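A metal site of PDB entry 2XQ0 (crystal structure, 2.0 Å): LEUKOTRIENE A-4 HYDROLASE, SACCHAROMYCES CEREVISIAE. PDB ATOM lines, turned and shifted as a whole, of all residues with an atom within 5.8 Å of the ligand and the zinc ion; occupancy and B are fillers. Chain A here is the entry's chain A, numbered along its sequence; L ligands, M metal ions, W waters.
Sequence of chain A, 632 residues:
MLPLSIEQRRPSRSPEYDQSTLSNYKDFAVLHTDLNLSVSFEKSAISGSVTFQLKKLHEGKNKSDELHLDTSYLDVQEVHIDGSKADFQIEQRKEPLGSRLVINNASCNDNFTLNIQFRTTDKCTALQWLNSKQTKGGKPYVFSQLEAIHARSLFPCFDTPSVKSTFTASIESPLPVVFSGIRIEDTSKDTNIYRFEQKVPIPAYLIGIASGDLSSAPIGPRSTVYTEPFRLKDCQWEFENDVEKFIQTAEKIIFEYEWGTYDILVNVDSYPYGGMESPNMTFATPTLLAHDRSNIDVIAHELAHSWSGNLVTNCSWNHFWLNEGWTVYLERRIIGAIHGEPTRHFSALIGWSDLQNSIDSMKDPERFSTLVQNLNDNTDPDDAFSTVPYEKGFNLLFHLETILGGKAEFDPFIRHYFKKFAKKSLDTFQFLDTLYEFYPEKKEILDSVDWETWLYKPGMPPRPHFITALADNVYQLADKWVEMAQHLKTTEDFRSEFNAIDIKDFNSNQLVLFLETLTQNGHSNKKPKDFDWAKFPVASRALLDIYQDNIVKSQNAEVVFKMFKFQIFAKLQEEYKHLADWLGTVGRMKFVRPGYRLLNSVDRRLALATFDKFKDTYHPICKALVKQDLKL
O1 of the ligand lies close to OE2 of Glu 302, at 3.2 Å. N of Gly 274 lies within hydrogen-bond range of O4 of the ligand. OE1 of Glu 277 lies within salt-bridge range of N1 of the ligand (2.8 Å). OH of Tyr 390 sits close to O2 of the ligand. SD of Met 276 lies within hydrogen-bond range of N1 of the ligand (3.1 Å). N1 of the ligand lies within salt-bridge range of OE1 of Glu 147 (2.8 Å). O4 of the ligand sits at hydrogen-bond distance from N of Gly 275, 3.4 Å away.
Of the 23 residues printed, 3 come within 4 Å of the zinc ion.
OE2 of Glu 302 sits at hydrogen-bond distance from N of Glu 277 (3.2 Å). The backbone NH (N) of Glu 147 sits close to the side-chain amide nitrogen (NE2) of Gln 145, at 3.1 Å. ND1 of His 301 is in hydrogen-bond range of OE1 of Glu 331, at 2.7 Å. ND1 of His 305 sits at hydrogen-bond distance from OG1 of Thr 327.
Water W1 lies within hydrogen-bond range of the guanidinium group of Arg 588 (2.6 Å), an oxygen (O3) of the ligand (2.7 Å) and the backbone NH of Gly 274 (3.1 Å).
The zinc ion is bound by a ring nitrogen (NE2) of His 305 (2.0 Å), a ring nitrogen (NE2) of His 301 (2.2 Å), the side-chain carboxylate of Glu 324 (2.2 Å), an oxygen (O1) of the ligand (2.4 Å) and an oxygen (O2) of the ligand (2.4 Å). The zinc ion has five donor atoms within binding distance. Slightly farther from the zinc ion lies OE2 of Glu 324 (2.7 Å).
Tyr 273 touches the ligand (CB to O4, 3.3 Å). CZ of Phe 320 touches C6 of the ligand, at 3.8 Å. Hydrophobic or aromatic side chains that line the ligand: Tyr 273, Met 276, His 301, His 305, Phe 320 and Tyr 390. The nearest printed residue that does not touch the ligand is Phe 385 (4.02 Å).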
ATOM      1  N   GLN A 145       7.765  17.328 -19.214  1.00  0.00           N
ATOM      2  CA  GLN A 145       8.285  17.438 -17.864  1.00  0.00           C
ATOM      3  C   GLN A 145       9.532  16.560 -17.871  1.00  0.00           C
ATOM      4  O   GLN A 145       9.417  15.331 -17.966  1.00  0.00           O
ATOM      5  CB  GLN A 145       7.265  16.935 -16.844  1.00  0.00           C
ATOM      6  CG  GLN A 145       7.871  16.621 -15.476  1.00  0.00           C
ATOM      7  CD  GLN A 145       8.507  17.839 -14.839  1.00  0.00           C
ATOM      8  OE1 GLN A 145       7.855  18.876 -14.707  1.00  0.00           O
ATOM      9  NE2 GLN A 145       9.771  17.722 -14.457  1.00  0.00           N
ATOM     10  N   GLU A 147      12.474  16.765 -15.715  1.00  0.00           N
ATOM     11  CA  GLU A 147      13.255  16.493 -14.492  1.00  0.00           C
ATOM     12  C   GLU A 147      12.804  15.159 -13.901  1.00  0.00           C
ATOM     13  O   GLU A 147      11.605  14.911 -13.840  1.00  0.00           O
ATOM     14  CB  GLU A 147      13.061  17.609 -13.464  1.00  0.00           C
ATOM     15  CG  GLU A 147      14.126  17.642 -12.357  1.00  0.00           C
ATOM     16  CD  GLU A 147      13.949  18.869 -11.468  1.00  0.00           C
ATOM     17  OE1 GLU A 147      13.055  19.669 -11.771  1.00  0.00           O
ATOM     18  OE2 GLU A 147      14.679  19.032 -10.473  1.00  0.00           O
ATOM     19  N   ALA A 148      13.743  14.300 -13.488  1.00  0.00           N
ATOM     20  CA  ALA A 148      15.174  14.559 -13.495  1.00  0.00           C
ATOM     21  C   ALA A 148      15.890  14.049 -14.748  1.00  0.00           C
ATOM     22  O   ALA A 148      16.725  14.769 -15.308  1.00  0.00           O
ATOM     23  CB  ALA A 148      15.822  13.939 -12.267  1.00  0.00           C
ATOM     24  N   PRO A 272       0.842  17.319 -13.164  1.00  0.00           N
ATOM     25  CA  PRO A 272       1.060  16.549 -11.926  1.00  0.00           C
ATOM     26  C   PRO A 272       1.910  17.225 -10.844  1.00  0.00           C
ATOM     27  O   PRO A 272       1.938  16.728  -9.718  1.00  0.00           O
ATOM     28  CB  PRO A 272       1.788  15.299 -12.446  1.00  0.00           C
ATOM     29  CG  PRO A 272       2.590  15.816 -13.608  1.00  0.00           C
ATOM     30  CD  PRO A 272       1.813  16.960 -14.214  1.00  0.00           C
ATOM     31  N   TYR A 273       2.606  18.312 -11.157  1.00  0.00           N
ATOM     32  CA  TYR A 273       3.407  19.000 -10.157  1.00  0.00           C
ATOM     33  C   TYR A 273       2.772  20.338  -9.844  1.00  0.00           C
ATOM     34  O   TYR A 273       1.793  20.719 -10.482  1.00  0.00           O
ATOM     35  CB  TYR A 273       4.862  19.151 -10.619  1.00  0.00           C
ATOM     36  CG  TYR A 273       5.501  17.809 -10.895  1.00  0.00           C
ATOM     37  CD1 TYR A 273       6.155  17.111  -9.893  1.00  0.00           C
ATOM     38  CD2 TYR A 273       5.410  17.222 -12.152  1.00  0.00           C
ATOM     39  CE1 TYR A 273       6.730  15.878 -10.142  1.00  0.00           C
ATOM     40  CE2 TYR A 273       5.976  15.993 -12.402  1.00  0.00           C
ATOM     41  CZ  TYR A 273       6.631  15.320 -11.403  1.00  0.00           C
ATOM     42  OH  TYR A 273       7.197  14.090 -11.653  1.00  0.00           O
ATOM     43  N   GLY A 274       3.302  21.023  -8.838  1.00  0.00           N
ATOM     44  CA  GLY A 274       2.786  22.324  -8.461  1.00  0.00           C
ATOM     45  C   GLY A 274       3.370  23.299  -9.467  1.00  0.00           C
ATOM     46  O   GLY A 274       2.717  24.237  -9.897  1.00  0.00           O
ATOM     47  N   GLY A 275       4.604  23.048  -9.880  1.00  0.00           N
ATOM     48  CA  GLY A 275       5.268  23.925 -10.827  1.00  0.00           C
ATOM     49  C   GLY A 275       6.558  23.326 -11.311  1.00  0.00           C
ATOM     50  O   GLY A 275       7.049  22.376 -10.720  1.00  0.00           O
ATOM     51  N   MET A 276       7.110  23.882 -12.390  1.00  0.00           N
ATOM     52  CA  MET A 276       8.408  23.432 -12.905  1.00  0.00           C
ATOM     53  C   MET A 276       9.068  24.690 -13.410  1.00  0.00           C
ATOM     54  O   MET A 276       8.481  25.427 -14.199  1.00  0.00           O
ATOM     55  CB  MET A 276       8.272  22.434 -14.038  1.00  0.00           C
ATOM     56  CG  MET A 276       9.589  22.028 -14.688  1.00  0.00           C
ATOM     57  SD  MET A 276      10.791  21.310 -13.529  1.00  0.00           S
ATOM     58  CE  MET A 276      12.353  21.784 -14.292  1.00  0.00           C
ATOM     59  N   GLU A 277      10.303  24.908 -12.954  1.00  0.00           N
ATOM     60  CA  GLU A 277      11.035  26.145 -13.174  1.00  0.00           C
ATOM     61  C   GLU A 277      11.768  26.232 -14.516  1.00  0.00           C
ATOM     62  O   GLU A 277      12.916  26.681 -14.561  1.00  0.00           O
ATOM     63  CB  GLU A 277      12.068  26.281 -12.042  1.00  0.00           C
ATOM     64  CG  GLU A 277      13.247  25.247 -12.098  1.00  0.00           C
ATOM     65  CD  GLU A 277      12.994  23.949 -11.288  1.00  0.00           C
ATOM     66  OE1 GLU A 277      11.827  23.605 -10.986  1.00  0.00           O
ATOM     67  OE2 GLU A 277      13.991  23.260 -10.949  1.00  0.00           O
ATOM     68  N   ASP A 297       2.774  31.445  -3.459  1.00  0.00           N
ATOM     69  CA  ASP A 297       4.130  31.214  -3.011  1.00  0.00           C
ATOM     70  C   ASP A 297       4.784  30.145  -3.897  1.00  0.00           C
ATOM     71  O   ASP A 297       5.997  30.127  -4.083  1.00  0.00           O
ATOM     72  CB  ASP A 297       4.117  30.825  -1.545  1.00  0.00           C
ATOM     73  CG  ASP A 297       3.233  31.748  -0.714  1.00  0.00           C
ATOM     74  OD1 ASP A 297       2.866  32.838  -1.230  1.00  0.00           O
ATOM     75  OD2 ASP A 297       2.888  31.385   0.432  1.00  0.00           O
ATOM     76  N   VAL A 298       3.969  29.268  -4.478  1.00  0.00           N
ATOM     77  CA  VAL A 298       4.507  28.309  -5.438  1.00  0.00           C
ATOM     78  C   VAL A 298       5.218  29.075  -6.547  1.00  0.00           C
ATOM     79  O   VAL A 298       6.139  28.544  -7.184  1.00  0.00           O
ATOM     80  CB  VAL A 298       3.420  27.412  -6.061  1.00  0.00           C
ATOM     81  CG1 VAL A 298       4.032  26.521  -7.154  1.00  0.00           C
ATOM     82  CG2 VAL A 298       2.733  26.573  -4.981  1.00  0.00           C
ATOM     83  N   HIS A 301       8.591  30.171  -5.220  1.00  0.00           N
ATOM     84  CA  HIS A 301       9.430  28.988  -5.349  1.00  0.00           C
ATOM     85  C   HIS A 301      10.058  28.863  -6.737  1.00  0.00           C
ATOM     86  O   HIS A 301      11.264  28.848  -6.866  1.00  0.00           O
ATOM     87  CB  HIS A 301       8.660  27.710  -5.005  1.00  0.00           C
ATOM     88  CG  HIS A 301       9.549  26.504  -4.929  1.00  0.00           C
ATOM     89  ND1 HIS A 301      10.163  26.098  -3.766  1.00  0.00           N
ATOM     90  CD2 HIS A 301       9.957  25.643  -5.893  1.00  0.00           C
ATOM     91  CE1 HIS A 301      10.905  25.029  -4.008  1.00  0.00           C
ATOM     92  NE2 HIS A 301      10.802  24.735  -5.297  1.00  0.00           N
ATOM     93  N   GLU A 302       9.235  28.771  -7.785  1.00  0.00           N
ATOM     94  CA  GLU A 302       9.773  28.634  -9.129  1.00  0.00           C
ATOM     95  C   GLU A 302      10.632  29.837  -9.489  1.00  0.00           C
ATOM     96  O   GLU A 302      11.616  29.718 -10.215  1.00  0.00           O
ATOM     97  CB  GLU A 302       8.645  28.537 -10.165  1.00  0.00           C
ATOM     98  CG  GLU A 302       7.557  27.523  -9.839  1.00  0.00           C
ATOM     99  CD  GLU A 302       8.098  26.136  -9.652  1.00  0.00           C
ATOM    100  OE1 GLU A 302       7.391  25.304  -9.032  1.00  0.00           O
ATOM    101  OE2 GLU A 302       9.238  25.863 -10.098  1.00  0.00           O
ATOM    102  N   HIS A 305      14.190  29.541  -8.166  1.00  0.00           N
ATOM    103  CA  HIS A 305      14.957  28.611  -8.988  1.00  0.00           C
ATOM    104  C   HIS A 305      15.774  29.328 -10.060  1.00  0.00           C
ATOM    105  O   HIS A 305      16.838  28.854 -10.492  1.00  0.00           O
ATOM    106  CB  HIS A 305      14.038  27.583  -9.663  1.00  0.00           C
ATOM    107  CG  HIS A 305      13.835  26.339  -8.869  1.00  0.00           C
ATOM    108  ND1 HIS A 305      14.886  25.590  -8.396  1.00  0.00           N
ATOM    109  CD2 HIS A 305      12.697  25.709  -8.471  1.00  0.00           C
ATOM    110  CE1 HIS A 305      14.409  24.555  -7.722  1.00  0.00           C
ATOM    111  NE2 HIS A 305      13.088  24.609  -7.753  1.00  0.00           N
ATOM    112  N   PHE A 320      21.266  17.073  -5.061  1.00  0.00           N
ATOM    113  CA  PHE A 320      19.990  17.720  -5.382  1.00  0.00           C
ATOM    114  C   PHE A 320      19.610  18.778  -4.340  1.00  0.00           C
ATOM    115  O   PHE A 320      18.902  19.732  -4.655  1.00  0.00           O
ATOM    116  CB  PHE A 320      18.909  16.643  -5.477  1.00  0.00           C
ATOM    117  CG  PHE A 320      17.583  17.136  -5.968  1.00  0.00           C
ATOM    118  CD1 PHE A 320      17.498  17.928  -7.120  1.00  0.00           C
ATOM    119  CD2 PHE A 320      16.399  16.763  -5.330  1.00  0.00           C
ATOM    120  CE1 PHE A 320      16.266  18.366  -7.593  1.00  0.00           C
ATOM    121  CE2 PHE A 320      15.164  17.198  -5.789  1.00  0.00           C
ATOM    122  CZ  PHE A 320      15.106  18.001  -6.940  1.00  0.00           C
ATOM    123  N   GLU A 324      17.153  22.294  -4.502  1.00  0.00           N
ATOM    124  CA  GLU A 324      15.888  22.456  -3.773  1.00  0.00           C
ATOM    125  C   GLU A 324      16.023  23.082  -2.382  1.00  0.00           C
ATOM    126  O   GLU A 324      15.139  23.793  -1.941  1.00  0.00           O
ATOM    127  CB  GLU A 324      15.127  21.138  -3.698  1.00  0.00           C
ATOM    128  CG  GLU A 324      14.678  20.587  -5.066  1.00  0.00           C
ATOM    129  CD  GLU A 324      13.731  21.518  -5.814  1.00  0.00           C
ATOM    130  OE1 GLU A 324      13.146  22.441  -5.202  1.00  0.00           O
ATOM    131  OE2 GLU A 324      13.549  21.313  -7.038  1.00  0.00           O
ATOM    132  N   THR A 327      16.558  26.776  -2.949  1.00  0.00           N
ATOM    133  CA  THR A 327      15.286  27.343  -3.422  1.00  0.00           C
ATOM    134  C   THR A 327      14.292  27.562  -2.284  1.00  0.00           C
ATOM    135  O   THR A 327      13.690  28.621  -2.197  1.00  0.00           O
ATOM    136  CB  THR A 327      14.654  26.484  -4.532  1.00  0.00           C
ATOM    137  OG1 THR A 327      15.580  26.413  -5.631  1.00  0.00           O
ATOM    138  CG2 THR A 327      13.312  27.085  -5.016  1.00  0.00           C
ATOM    139  N   VAL A 328      14.117  26.559  -1.427  1.00  0.00           N
ATOM    140  CA  VAL A 328      13.176  26.668  -0.325  1.00  0.00           C
ATOM    141  C   VAL A 328      13.642  27.783   0.609  1.00  0.00           C
ATOM    142  O   VAL A 328      12.831  28.574   1.110  1.00  0.00           O
ATOM    143  CB  VAL A 328      12.996  25.301   0.446  1.00  0.00           C
ATOM    144  CG1 VAL A 328      12.116  25.487   1.692  1.00  0.00           C
ATOM    145  CG2 VAL A 328      12.375  24.218  -0.474  1.00  0.00           C
ATOM    146  N   GLU A 331      12.990  31.138  -1.322  1.00  0.00           N
ATOM    147  CA  GLU A 331      11.540  31.320  -1.352  1.00  0.00           C
ATOM    148  C   GLU A 331      11.057  31.917  -0.032  1.00  0.00           C
ATOM    149  O   GLU A 331      10.308  32.883  -0.009  1.00  0.00           O
ATOM    150  CB  GLU A 331      10.879  29.945  -1.552  1.00  0.00           C
ATOM    151  CG  GLU A 331       9.362  29.880  -1.390  1.00  0.00           C
ATOM    152  CD  GLU A 331       8.844  28.430  -1.343  1.00  0.00           C
ATOM    153  OE1 GLU A 331       9.669  27.479  -1.457  1.00  0.00           O
ATOM    154  OE2 GLU A 331       7.619  28.253  -1.180  1.00  0.00           O
ATOM    155  N   ASP A 382      14.602   9.314  -9.194  1.00  0.00           N
ATOM    156  CA  ASP A 382      13.293   9.513  -8.586  1.00  0.00           C
ATOM    157  C   ASP A 382      13.281   8.970  -7.169  1.00  0.00           C
ATOM    158  O   ASP A 382      12.781   9.622  -6.255  1.00  0.00           O
ATOM    159  CB  ASP A 382      12.197   8.780  -9.388  1.00  0.00           C
ATOM    160  CG  ASP A 382      11.649   9.608 -10.543  1.00  0.00           C
ATOM    161  OD1 ASP A 382      11.736  10.856 -10.502  1.00  0.00           O
ATOM    162  OD2 ASP A 382      11.119   9.006 -11.504  1.00  0.00           O
ATOM    163  N   PHE A 385      14.031  11.366  -4.482  1.00  0.00           N
ATOM    164  CA  PHE A 385      13.300  12.605  -4.296  1.00  0.00           C
ATOM    165  C   PHE A 385      12.278  12.406  -3.186  1.00  0.00           C
ATOM    166  O   PHE A 385      11.505  11.448  -3.162  1.00  0.00           O
ATOM    167  CB  PHE A 385      12.674  13.105  -5.607  1.00  0.00           C
ATOM    168  CG  PHE A 385      13.688  13.365  -6.693  1.00  0.00           C
ATOM    169  CD1 PHE A 385      14.938  13.878  -6.380  1.00  0.00           C
ATOM    170  CD2 PHE A 385      13.405  13.057  -8.018  1.00  0.00           C
ATOM    171  CE1 PHE A 385      15.880  14.106  -7.378  1.00  0.00           C
ATOM    172  CE2 PHE A 385      14.348  13.290  -9.007  1.00  0.00           C
ATOM    173  CZ  PHE A 385      15.576  13.804  -8.691  1.00  0.00           C
ATOM    174  N   TYR A 390      14.589  19.315   0.199  1.00  0.00           N
ATOM    175  CA  TYR A 390      13.908  20.585   0.372  1.00  0.00           C
ATOM    176  C   TYR A 390      14.104  21.112   1.789  1.00  0.00           C
ATOM    177  O   TYR A 390      14.627  22.202   2.003  1.00  0.00           O
ATOM    178  CB  TYR A 390      12.400  20.411   0.104  1.00  0.00           C
ATOM    179  CG  TYR A 390      12.057  20.082  -1.340  1.00  0.00           C
ATOM    180  CD1 TYR A 390      12.121  18.766  -1.807  1.00  0.00           C
ATOM    181  CD2 TYR A 390      11.648  21.074  -2.213  1.00  0.00           C
ATOM    182  CE1 TYR A 390      11.809  18.465  -3.144  1.00  0.00           C
ATOM    183  CE2 TYR A 390      11.338  20.779  -3.541  1.00  0.00           C
ATOM    184  CZ  TYR A 390      11.422  19.483  -4.001  1.00  0.00           C
ATOM    185  OH  TYR A 390      11.096  19.207  -5.314  1.00  0.00           O
ATOM    186  N   ARG A 588      -3.027  17.083 -10.054  1.00  0.00           N
ATOM    187  CA  ARG A 588      -1.832  17.324  -9.242  1.00  0.00           C
ATOM    188  C   ARG A 588      -1.582  16.168  -8.271  1.00  0.00           C
ATOM    189  O   ARG A 588      -2.434  15.868  -7.442  1.00  0.00           O
ATOM    190  CB  ARG A 588      -1.969  18.646  -8.474  1.00  0.00           C
ATOM    191  CG  ARG A 588      -0.703  19.060  -7.740  1.00  0.00           C
ATOM    192  CD  ARG A 588      -0.818  20.476  -7.208  1.00  0.00           C
ATOM    193  NE  ARG A 588       0.375  20.876  -6.479  1.00  0.00           N
ATOM    194  CZ  ARG A 588       0.491  21.985  -5.772  1.00  0.00           C
ATOM    195  NH1 ARG A 588      -0.520  22.838  -5.703  1.00  0.00           N
ATOM    196  NH2 ARG A 588       1.622  22.253  -5.132  1.00  0.00           N
HETATM  197  N1  LIG L   1      10.928  21.045 -10.493  1.00  0.00           N
HETATM  198  C1  LIG L   1      10.415  20.860  -9.148  1.00  0.00           C
HETATM  199  C2  LIG L   1       9.477  19.656  -9.093  1.00  0.00           C
HETATM  200  C3  LIG L   1      10.240  18.394  -9.423  1.00  0.00           C
HETATM  201  C4  LIG L   1      11.463  18.140  -8.825  1.00  0.00           C
HETATM  202  C5  LIG L   1       9.717  17.492 -10.347  1.00  0.00           C
HETATM  203  C6  LIG L   1      12.171  16.982  -9.126  1.00  0.00           C
HETATM  204  C7  LIG L   1      10.424  16.329 -10.657  1.00  0.00           C
HETATM  205  C8  LIG L   1      11.644  16.072 -10.045  1.00  0.00           C
HETATM  206  C9  LIG L   1       9.695  22.121  -8.647  1.00  0.00           C
HETATM  207  O1  LIG L   1      10.483  23.320  -8.677  1.00  0.00           O
HETATM  208  C10 LIG L   1       9.256  21.849  -7.249  1.00  0.00           C
HETATM  209  O2  LIG L   1      10.055  21.809  -6.319  1.00  0.00           O
HETATM  210  N2  LIG L   1       7.939  21.651  -7.213  1.00  0.00           N
HETATM  211  C11 LIG L   1       7.111  21.355  -6.061  1.00  0.00           C
HETATM  212  C12 LIG L   1       6.554  22.717  -5.668  1.00  0.00           C
HETATM  213  C13 LIG L   1       6.787  23.056  -4.202  1.00  0.00           C
HETATM  214  C14 LIG L   1       6.706  24.563  -3.999  1.00  0.00           C
HETATM  215  C15 LIG L   1       8.118  22.508  -3.690  1.00  0.00           C
HETATM  216  C16 LIG L   1       5.996  20.488  -6.546  1.00  0.00           C
HETATM  217  O3  LIG L   1       5.432  19.705  -5.752  1.00  0.00           O
HETATM  218  O4  LIG L   1       5.662  20.578  -7.760  1.00  0.00           O
HETATM  219 ZN    ZN M   1      11.805  23.392  -6.727  1.00  0.00          ZN
HETATM  220  O   HOH W   1       2.713  19.827  -6.093  1.00  0.00           O
